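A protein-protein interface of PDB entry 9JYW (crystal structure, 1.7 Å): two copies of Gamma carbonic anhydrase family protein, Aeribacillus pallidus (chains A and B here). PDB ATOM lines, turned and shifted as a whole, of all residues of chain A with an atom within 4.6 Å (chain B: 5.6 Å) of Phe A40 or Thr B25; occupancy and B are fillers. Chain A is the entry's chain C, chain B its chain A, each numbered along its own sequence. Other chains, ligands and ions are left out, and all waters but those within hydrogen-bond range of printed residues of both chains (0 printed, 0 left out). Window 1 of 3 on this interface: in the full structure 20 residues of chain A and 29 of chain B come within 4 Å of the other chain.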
ATOM      1  N   TYR A  19       5.476 -26.764  23.724  1.00  0.00           N
ATOM      2  CA  TYR A  19       4.119 -26.229  23.938  1.00  0.00           C
ATOM      3  C   TYR A  19       4.060 -24.838  23.323  1.00  0.00           C
ATOM      4  O   TYR A  19       4.913 -24.031  23.698  1.00  0.00           O
ATOM      5  CB  TYR A  19       3.779 -26.178  25.422  1.00  0.00           C
ATOM      6  CG  TYR A  19       2.525 -25.404  25.766  1.00  0.00           C
ATOM      7  CD1 TYR A  19       1.325 -25.662  25.112  1.00  0.00           C
ATOM      8  CD2 TYR A  19       2.543 -24.395  26.706  1.00  0.00           C
ATOM      9  CE1 TYR A  19       0.169 -24.968  25.429  1.00  0.00           C
ATOM     10  CE2 TYR A  19       1.397 -23.690  27.042  1.00  0.00           C
ATOM     11  CZ  TYR A  19       0.211 -23.983  26.406  1.00  0.00           C
ATOM     12  OH  TYR A  19      -0.927 -23.270  26.708  1.00  0.00           O
ATOM     13  N   ALA A  21       1.341 -21.925  23.100  1.00  0.00           N
ATOM     14  CA  ALA A  21       0.075 -21.514  23.723  1.00  0.00           C
ATOM     15  C   ALA A  21      -0.834 -20.818  22.728  1.00  0.00           C
ATOM     16  O   ALA A  21      -0.404 -20.513  21.572  1.00  0.00           O
ATOM     17  CB  ALA A  21       0.366 -20.661  24.912  1.00  0.00           C
ATOM     18  N   ASP A  22      -2.049 -20.512  23.133  1.00  0.00           N
ATOM     19  CA  ASP A  22      -3.019 -19.720  22.331  1.00  0.00           C
ATOM     20  C   ASP A  22      -2.535 -18.290  22.111  1.00  0.00           C
ATOM     21  O   ASP A  22      -1.817 -17.762  22.960  1.00  0.00           O
ATOM     22  CB  ASP A  22      -4.397 -19.671  22.989  1.00  0.00           C
ATOM     23  CG  ASP A  22      -4.992 -21.056  23.094  1.00  0.00           C
ATOM     24  OD1 ASP A  22      -5.458 -21.524  22.063  1.00  0.00           O
ATOM     25  OD2 ASP A  22      -4.906 -21.687  24.184  1.00  0.00           O
ATOM     26  N   PHE A  23      -2.892 -17.734  20.952  1.00  0.00           N
ATOM     27  CA  PHE A  23      -2.621 -16.326  20.577  1.00  0.00           C
ATOM     28  C   PHE A  23      -1.120 -16.094  20.404  1.00  0.00           C
ATOM     29  O   PHE A  23      -0.703 -14.930  20.445  1.00  0.00           O
ATOM     30  CB  PHE A  23      -3.176 -15.355  21.623  1.00  0.00           C
ATOM     31  CG  PHE A  23      -4.630 -15.566  21.945  1.00  0.00           C
ATOM     32  CD1 PHE A  23      -5.570 -15.616  20.920  1.00  0.00           C
ATOM     33  CD2 PHE A  23      -5.059 -15.737  23.247  1.00  0.00           C
ATOM     34  CE1 PHE A  23      -6.918 -15.820  21.193  1.00  0.00           C
ATOM     35  CE2 PHE A  23      -6.406 -15.900  23.516  1.00  0.00           C
ATOM     36  CZ  PHE A  23      -7.332 -15.943  22.496  1.00  0.00           C
ATOM     37  N   VAL A  24      -0.340 -17.160  20.193  1.00  0.00           N
ATOM     38  CA  VAL A  24       1.109 -17.040  19.899  1.00  0.00           C
ATOM     39  C   VAL A  24       1.286 -16.854  18.387  1.00  0.00           C
ATOM     40  O   VAL A  24       0.557 -17.524  17.605  1.00  0.00           O
ATOM     41  CB  VAL A  24       1.894 -18.237  20.433  1.00  0.00           C
ATOM     42  CG1 VAL A  24       3.321 -18.271  19.887  1.00  0.00           C
ATOM     43  CG2 VAL A  24       1.900 -18.221  21.948  1.00  0.00           C
ATOM     44  N   ILE A  38       6.285 -21.780  24.771  1.00  0.00           N
ATOM     45  CA  ILE A  38       6.053 -20.369  24.337  1.00  0.00           C
ATOM     46  C   ILE A  38       4.639 -20.016  24.806  1.00  0.00           C
ATOM     47  O   ILE A  38       3.646 -20.623  24.323  1.00  0.00           O
ATOM     48  CB  ILE A  38       6.185 -20.213  22.822  1.00  0.00           C
ATOM     49  CG1 ILE A  38       7.448 -20.864  22.247  1.00  0.00           C
ATOM     50  CG2 ILE A  38       6.088 -18.738  22.472  1.00  0.00           C
ATOM     51  CD1 ILE A  38       8.744 -20.367  22.844  1.00  0.00           C
ATOM     52  N   TRP A  39       4.544 -19.090  25.744  1.00  0.00           N
ATOM     53  CA  TRP A  39       3.299 -18.844  26.510  1.00  0.00           C
ATOM     54  C   TRP A  39       2.438 -17.774  25.826  1.00  0.00           C
ATOM     55  O   TRP A  39       2.845 -17.159  24.841  1.00  0.00           O
ATOM     56  CB  TRP A  39       3.644 -18.559  27.983  1.00  0.00           C
ATOM     57  CG  TRP A  39       4.136 -19.797  28.651  1.00  0.00           C
ATOM     58  CD1 TRP A  39       5.396 -20.332  28.586  1.00  0.00           C
ATOM     59  CD2 TRP A  39       3.330 -20.747  29.361  1.00  0.00           C
ATOM     60  NE1 TRP A  39       5.437 -21.526  29.245  1.00  0.00           N
ATOM     61  CE2 TRP A  39       4.186 -21.812  29.738  1.00  0.00           C
ATOM     62  CE3 TRP A  39       1.986 -20.777  29.730  1.00  0.00           C
ATOM     63  CZ2 TRP A  39       3.717 -22.903  30.464  1.00  0.00           C
ATOM     64  CZ3 TRP A  39       1.535 -21.856  30.456  1.00  0.00           C
ATOM     65  CH2 TRP A  39       2.386 -22.913  30.807  1.00  0.00           C
ATOM     66  N   PHE A  40       1.232 -17.602  26.335  1.00  0.00           N
ATOM     67  CA  PHE A  40       0.128 -16.846  25.691  1.00  0.00           C
ATOM     68  C   PHE A  40       0.587 -15.468  25.217  1.00  0.00           C
ATOM     69  O   PHE A  40       1.250 -14.729  25.979  1.00  0.00           O
ATOM     70  CB  PHE A  40      -1.010 -16.715  26.702  1.00  0.00           C
ATOM     71  CG  PHE A  40      -1.581 -18.059  27.070  1.00  0.00           C
ATOM     72  CD1 PHE A  40      -2.550 -18.632  26.280  1.00  0.00           C
ATOM     73  CD2 PHE A  40      -1.151 -18.733  28.201  1.00  0.00           C
ATOM     74  CE1 PHE A  40      -3.073 -19.881  26.594  1.00  0.00           C
ATOM     75  CE2 PHE A  40      -1.662 -19.976  28.512  1.00  0.00           C
ATOM     76  CZ  PHE A  40      -2.607 -20.555  27.686  1.00  0.00           C
ATOM     77  N   GLN A  41       0.143 -15.115  24.008  1.00  0.00           N
ATOM     78  CA  GLN A  41       0.218 -13.730  23.437  1.00  0.00           C
ATOM     79  C   GLN A  41       1.652 -13.395  23.001  1.00  0.00           C
ATOM     80  O   GLN A  41       1.895 -12.293  22.468  1.00  0.00           O
ATOM     81  CB  GLN A  41      -0.409 -12.731  24.436  1.00  0.00           C
ATOM     82  CG  GLN A  41      -1.949 -12.786  24.396  1.00  0.00           C
ATOM     83  CD  GLN A  41      -2.707 -12.582  25.678  1.00  0.00           C
ATOM     84  OE1 GLN A  41      -2.218 -11.912  26.595  1.00  0.00           O
ATOM     85  NE2 GLN A  41      -3.932 -13.139  25.743  1.00  0.00           N
ATOM     86  N   THR A  42       2.600 -14.313  23.079  1.00  0.00           N
ATOM     87  CA  THR A  42       3.997 -14.041  22.695  1.00  0.00           C
ATOM     88  C   THR A  42       4.114 -13.955  21.163  1.00  0.00           C
ATOM     89  O   THR A  42       3.416 -14.687  20.459  1.00  0.00           O
ATOM     90  CB  THR A  42       4.935 -15.097  23.304  1.00  0.00           C
ATOM     91  OG1 THR A  42       5.040 -14.727  24.677  1.00  0.00           O
ATOM     92  CG2 THR A  42       6.312 -15.154  22.679  1.00  0.00           C
ATOM     93  N   ASP A  61       4.507 -15.228  29.069  1.00  0.00           N
ATOM     94  CA  ASP A  61       3.388 -14.567  28.354  1.00  0.00           C
ATOM     95  C   ASP A  61       3.814 -13.175  27.864  1.00  0.00           C
ATOM     96  O   ASP A  61       4.548 -12.467  28.549  1.00  0.00           O
ATOM     97  CB  ASP A  61       2.162 -14.485  29.265  1.00  0.00           C
ATOM     98  CG  ASP A  61       2.026 -15.697  30.169  1.00  0.00           C
ATOM     99  OD1 ASP A  61       2.851 -15.845  31.110  1.00  0.00           O
ATOM    100  OD2 ASP A  61       1.170 -16.523  29.874  1.00  0.00           O
ATOM    101  N   GLN A  62       3.301 -12.785  26.698  1.00  0.00           N
ATOM    102  CA  GLN A  62       3.369 -11.401  26.177  1.00  0.00           C
ATOM    103  C   GLN A  62       4.819 -10.970  25.968  1.00  0.00           C
ATOM    104  O   GLN A  62       5.094  -9.770  26.075  1.00  0.00           O
ATOM    105  CB  GLN A  62       2.649 -10.472  27.157  1.00  0.00           C
ATOM    106  CG  GLN A  62       1.154 -10.736  27.173  1.00  0.00           C
ATOM    107  CD  GLN A  62       0.466  -9.868  28.200  1.00  0.00           C
ATOM    108  OE1 GLN A  62       1.105  -9.326  29.102  1.00  0.00           O
ATOM    109  NE2 GLN A  62      -0.835  -9.727  28.014  1.00  0.00           N
ATOM    110  N   MET B   2     -12.233 -15.267  23.402  1.00  0.00           N
ATOM    111  CA  MET B   2     -11.289 -15.502  24.480  1.00  0.00           C
ATOM    112  C   MET B   2     -11.049 -16.974  24.833  1.00  0.00           C
ATOM    113  O   MET B   2     -11.766 -17.841  24.384  1.00  0.00           O
ATOM    114  CB  MET B   2     -11.801 -14.842  25.711  1.00  0.00           C
ATOM    115  CG  MET B   2     -13.225 -15.196  26.017  1.00  0.00           C
ATOM    116  SD  MET B   2     -13.530 -16.437  27.267  1.00  0.00           S
ATOM    117  CE  MET B   2     -14.384 -17.652  26.255  1.00  0.00           C
ATOM    118  N   VAL B   3     -10.018 -17.231  25.622  1.00  0.00           N
ATOM    119  CA  VAL B   3      -9.721 -18.588  26.056  1.00  0.00           C
ATOM    120  C   VAL B   3      -9.851 -18.721  27.581  1.00  0.00           C
ATOM    121  O   VAL B   3      -9.286 -17.950  28.302  1.00  0.00           O
ATOM    122  CB  VAL B   3      -8.318 -19.055  25.556  1.00  0.00           C
ATOM    123  CG1 VAL B   3      -7.771 -20.175  26.413  1.00  0.00           C
ATOM    124  CG2 VAL B   3      -8.381 -19.424  24.090  1.00  0.00           C
ATOM    125  N   ILE B   4     -10.654 -19.677  28.035  1.00  0.00           N
ATOM    126  CA  ILE B   4     -10.851 -19.926  29.465  1.00  0.00           C
ATOM    127  C   ILE B   4     -10.575 -21.400  29.740  1.00  0.00           C
ATOM    128  O   ILE B   4     -11.258 -22.258  29.214  1.00  0.00           O
ATOM    129  CB  ILE B   4     -12.280 -19.611  29.924  1.00  0.00           C
ATOM    130  CG1 ILE B   4     -12.672 -18.187  29.573  1.00  0.00           C
ATOM    131  CG2 ILE B   4     -12.412 -19.826  31.419  1.00  0.00           C
ATOM    132  CD1 ILE B   4     -12.041 -17.131  30.440  1.00  0.00           C
ATOM    133  N   TYR B   5      -9.565 -21.676  30.553  1.00  0.00           N
ATOM    134  CA  TYR B   5      -9.207 -23.046  30.853  1.00  0.00           C
ATOM    135  C   TYR B   5      -9.168 -23.364  32.320  1.00  0.00           C
ATOM    136  O   TYR B   5      -8.925 -22.486  33.110  1.00  0.00           O
ATOM    137  CB  TYR B   5      -7.767 -23.344  30.394  1.00  0.00           C
ATOM    138  CG  TYR B   5      -7.476 -23.368  28.909  1.00  0.00           C
ATOM    139  CD1 TYR B   5      -8.377 -23.893  28.008  1.00  0.00           C
ATOM    140  CD2 TYR B   5      -6.267 -22.908  28.421  1.00  0.00           C
ATOM    141  CE1 TYR B   5      -8.097 -23.929  26.654  1.00  0.00           C
ATOM    142  CE2 TYR B   5      -5.977 -22.940  27.073  1.00  0.00           C
ATOM    143  CZ  TYR B   5      -6.893 -23.455  26.191  1.00  0.00           C
ATOM    144  OH  TYR B   5      -6.603 -23.500  24.849  1.00  0.00           O
ATOM    145  N   PHE B  23      -9.347 -11.943  22.734  1.00  0.00           N
ATOM    146  CA  PHE B  23      -7.913 -12.284  22.851  1.00  0.00           C
ATOM    147  C   PHE B  23      -7.489 -12.323  24.317  1.00  0.00           C
ATOM    148  O   PHE B  23      -6.289 -12.218  24.592  1.00  0.00           O
ATOM    149  CB  PHE B  23      -7.041 -11.329  22.041  1.00  0.00           C
ATOM    150  CG  PHE B  23      -7.479 -11.143  20.606  1.00  0.00           C
ATOM    151  CD1 PHE B  23      -7.667 -12.236  19.785  1.00  0.00           C
ATOM    152  CD2 PHE B  23      -7.716  -9.883  20.081  1.00  0.00           C
ATOM    153  CE1 PHE B  23      -8.113 -12.078  18.480  1.00  0.00           C
ATOM    154  CE2 PHE B  23      -8.158  -9.734  18.777  1.00  0.00           C
ATOM    155  CZ  PHE B  23      -8.362 -10.828  17.988  1.00  0.00           C
ATOM    156  N   VAL B  24      -8.423 -12.431  25.252  1.00  0.00           N
ATOM    157  CA  VAL B  24      -8.119 -12.608  26.691  1.00  0.00           C
ATOM    158  C   VAL B  24      -7.927 -14.094  27.000  1.00  0.00           C
ATOM    159  O   VAL B  24      -8.700 -14.952  26.469  1.00  0.00           O
ATOM    160  CB  VAL B  24      -9.201 -11.956  27.562  1.00  0.00           C
ATOM    161  CG1 VAL B  24      -9.066 -12.353  29.027  1.00  0.00           C
ATOM    162  CG2 VAL B  24      -9.177 -10.447  27.404  1.00  0.00           C
ATOM    163  N   THR B  25      -6.922 -14.379  27.827  1.00  0.00           N
ATOM    164  CA  THR B  25      -6.694 -15.735  28.377  1.00  0.00           C
ATOM    165  C   THR B  25      -6.942 -15.693  29.890  1.00  0.00           C
ATOM    166  O   THR B  25      -6.267 -14.909  30.559  1.00  0.00           O
ATOM    167  CB  THR B  25      -5.260 -16.177  28.093  1.00  0.00           C
ATOM    168  OG1 THR B  25      -5.094 -16.215  26.675  1.00  0.00           O
ATOM    169  CG2 THR B  25      -4.962 -17.536  28.666  1.00  0.00           C
ATOM    170  N   ILE B  26      -7.808 -16.553  30.417  1.00  0.00           N
ATOM    171  CA  ILE B  26      -7.982 -16.728  31.886  1.00  0.00           C
ATOM    172  C   ILE B  26      -7.930 -18.221  32.180  1.00  0.00           C
ATOM    173  O   ILE B  26      -8.675 -18.972  31.547  1.00  0.00           O
ATOM    174  CB  ILE B  26      -9.313 -16.093  32.338  1.00  0.00           C
ATOM    175  CG1 ILE B  26      -9.366 -14.605  31.973  1.00  0.00           C
ATOM    176  CG2 ILE B  26      -9.527 -16.318  33.839  1.00  0.00           C
ATOM    177  CD1 ILE B  26     -10.676 -13.971  32.117  1.00  0.00           C
ATOM    178  N   THR B  27      -7.091 -18.630  33.108  1.00  0.00           N
ATOM    179  CA  THR B  27      -6.978 -20.060  33.487  1.00  0.00           C
ATOM    180  C   THR B  27      -7.013 -20.247  35.004  1.00  0.00           C
ATOM    181  O   THR B  27      -6.547 -19.382  35.761  1.00  0.00           O
ATOM    182  CB  THR B  27      -5.706 -20.708  32.915  1.00  0.00           C
ATOM    183  OG1 THR B  27      -4.598 -20.355  33.742  1.00  0.00           O
ATOM    184  CG2 THR B  27      -5.415 -20.295  31.493  1.00  0.00           C
ATOM    185  N   THR B  42      -5.236  -9.268  27.486  1.00  0.00           N
ATOM    186  CA  THR B  42      -4.792  -9.536  28.872  1.00  0.00           C
ATOM    187  C   THR B  42      -4.688 -11.048  29.131  1.00  0.00           C
ATOM    188  O   THR B  42      -5.520 -11.828  28.637  1.00  0.00           O
ATOM    189  CB  THR B  42      -5.707  -8.805  29.853  1.00  0.00           C
ATOM    190  OG1 THR B  42      -5.311  -7.433  29.729  1.00  0.00           O
ATOM    191  CG2 THR B  42      -5.578  -9.267  31.292  1.00  0.00           C
ATOM    192  N   VAL B  43      -3.737 -11.420  29.961  1.00  0.00           N
ATOM    193  CA  VAL B  43      -3.525 -12.813  30.428  1.00  0.00           C
ATOM    194  C   VAL B  43      -3.642 -12.848  31.956  1.00  0.00           C
ATOM    195  O   VAL B  43      -2.927 -12.111  32.625  1.00  0.00           O
ATOM    196  CB  VAL B  43      -2.145 -13.343  29.966  1.00  0.00           C
ATOM    197  CG1 VAL B  43      -0.992 -12.410  30.291  1.00  0.00           C
ATOM    198  CG2 VAL B  43      -1.952 -14.777  30.476  1.00  0.00           C
ATOM    199  N   ILE B  44      -4.508 -13.712  32.455  1.00  0.00           N
ATOM    200  CA  ILE B  44      -4.627 -14.013  33.903  1.00  0.00           C
ATOM    201  C   ILE B  44      -4.469 -15.515  34.071  1.00  0.00           C
ATOM    202  O   ILE B  44      -5.422 -16.246  33.775  1.00  0.00           O
ATOM    203  CB  ILE B  44      -5.962 -13.504  34.479  1.00  0.00           C
ATOM    204  CG1 ILE B  44      -6.267 -12.055  34.079  1.00  0.00           C
ATOM    205  CG2 ILE B  44      -5.914 -13.677  35.981  1.00  0.00           C
ATOM    206  CD1 ILE B  44      -7.584 -11.542  34.554  1.00  0.00           C
ATOM    207  N   ARG B  45      -3.278 -15.967  34.454  1.00  0.00           N
ATOM    208  CA  ARG B  45      -3.026 -17.418  34.627  1.00  0.00           C
ATOM    209  C   ARG B  45      -3.079 -17.725  36.113  1.00  0.00           C
ATOM    210  O   ARG B  45      -2.199 -17.276  36.833  1.00  0.00           O
ATOM    211  CB  ARG B  45      -1.687 -17.859  34.035  1.00  0.00           C
ATOM    212  CG  ARG B  45      -1.749 -18.120  32.548  1.00  0.00           C
ATOM    213  CD  ARG B  45      -0.626 -19.017  32.094  1.00  0.00           C
ATOM    214  NE  ARG B  45       0.662 -18.368  32.173  1.00  0.00           N
ATOM    215  CZ  ARG B  45       1.721 -18.797  32.842  1.00  0.00           C
ATOM    216  NH1 ARG B  45       1.643 -19.828  33.665  1.00  0.00           N
ATOM    217  NH2 ARG B  45       2.846 -18.102  32.770  1.00  0.00           N
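Phe A40 touches just these residues of chain B: Thr B25 (3.5 Å) and Arg B45 (3.9 Å). Of chain A, only Phe A23 (3.4 Å), Phe A40 (3.5 Å) and Gln A41 (3.4 Å) come within 4 Å of Thr B25. Of the printed residues of chain B, Phe A23 touches Val B3 (3.97 Å), Phe B23 (3.7 Å), Val B24 (3.9 Å) and Thr B25 (3.4 Å). Of the printed residues of chain A, Val B3 touches Asp A22 (3.9 Å) and Phe A23 (3.97 Å). The nearest residue of chain B that does not touch Phe A40 is Tyr B5 (4.2 Å). The nearest printed residue of chain A that does not touch Thr B25 is Asp A22 (5.1 Å).
The side-chain carboxylate of Asp A61 lies within salt-bridge range of the guanidinium group of Arg B45 (2.8 Å). The side-chain amide nitrogen of Gln A41 sits at hydrogen-bond distance from the side-chain hydroxyl of Thr B25, 3.4 Å away. NE2 of Gln A41 is in hydrogen-bond range of O of Phe B23 (2.8 Å). OH of Tyr B5 lies within hydrogen-bond range of OD2 of Asp A22.
The backbone carbonyl oxygen (O) of Thr B42 is in hydrogen-bond range of the backbone NH (N) of Thr B25 (3.0 Å). O of Thr B25 sits at hydrogen-bond distance from N of Ile B44. The backbone NH (N) of Ile B26 lies within hydrogen-bond range of the backbone carbonyl oxygen (O) of Val B3, 2.9 Å away. The backbone NH of Tyr B5 is in hydrogen-bond range of the backbone carbonyl oxygen of Ile B26, at 3.0 Å. The backbone carbonyl oxygen (O) of Trp A39 sits at hydrogen-bond distance from the side-chain hydroxyl (OG1) of Thr A42. OG1 of Thr A42 sits at hydrogen-bond distance from N of Gln A62, at 3.3 Å.
Asp A22 touches Val B3. CG2 of Val B3 touches CZ of Phe A23, at 3.97 Å. CA of Phe B23 touches CZ of Phe A23, 3.7 Å away. Phe A23 touches Val B24. Trp A39 touches Arg B45. Thr B25 touches Phe A40. Arg B45 touches Phe A40 (CD to CE2, 3.9 Å). OE1 of Gln A41 touches CB of Val B43, at 3.7 Å. Asp A61 touches Val B43. CG1 of Val B43 touches NE2 of Gln A62, 3.5 Å away.
Hydrophobic or aromatic side chains of chain B within 4 Å of the printed part of chain A: Val B3, Tyr B5, Phe B23 and Val B43. Among the printed residues, Asp or Glu carboxylates within 4 Å of a Lys or Arg side-chain nitrogen of the other chain: Asp A61 with Arg B45.
Phe B23 touches its own counterpart, Phe A23. Phe A23 touches Val B24, but with the chains exchanged Val A24 does not touch Phe B23 (8.8 Å). 3 positions are printed for both chains. Of the 16 pairs that touch across the chains among the printed residues, 1 has its exchanged pair printed and touching as well.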
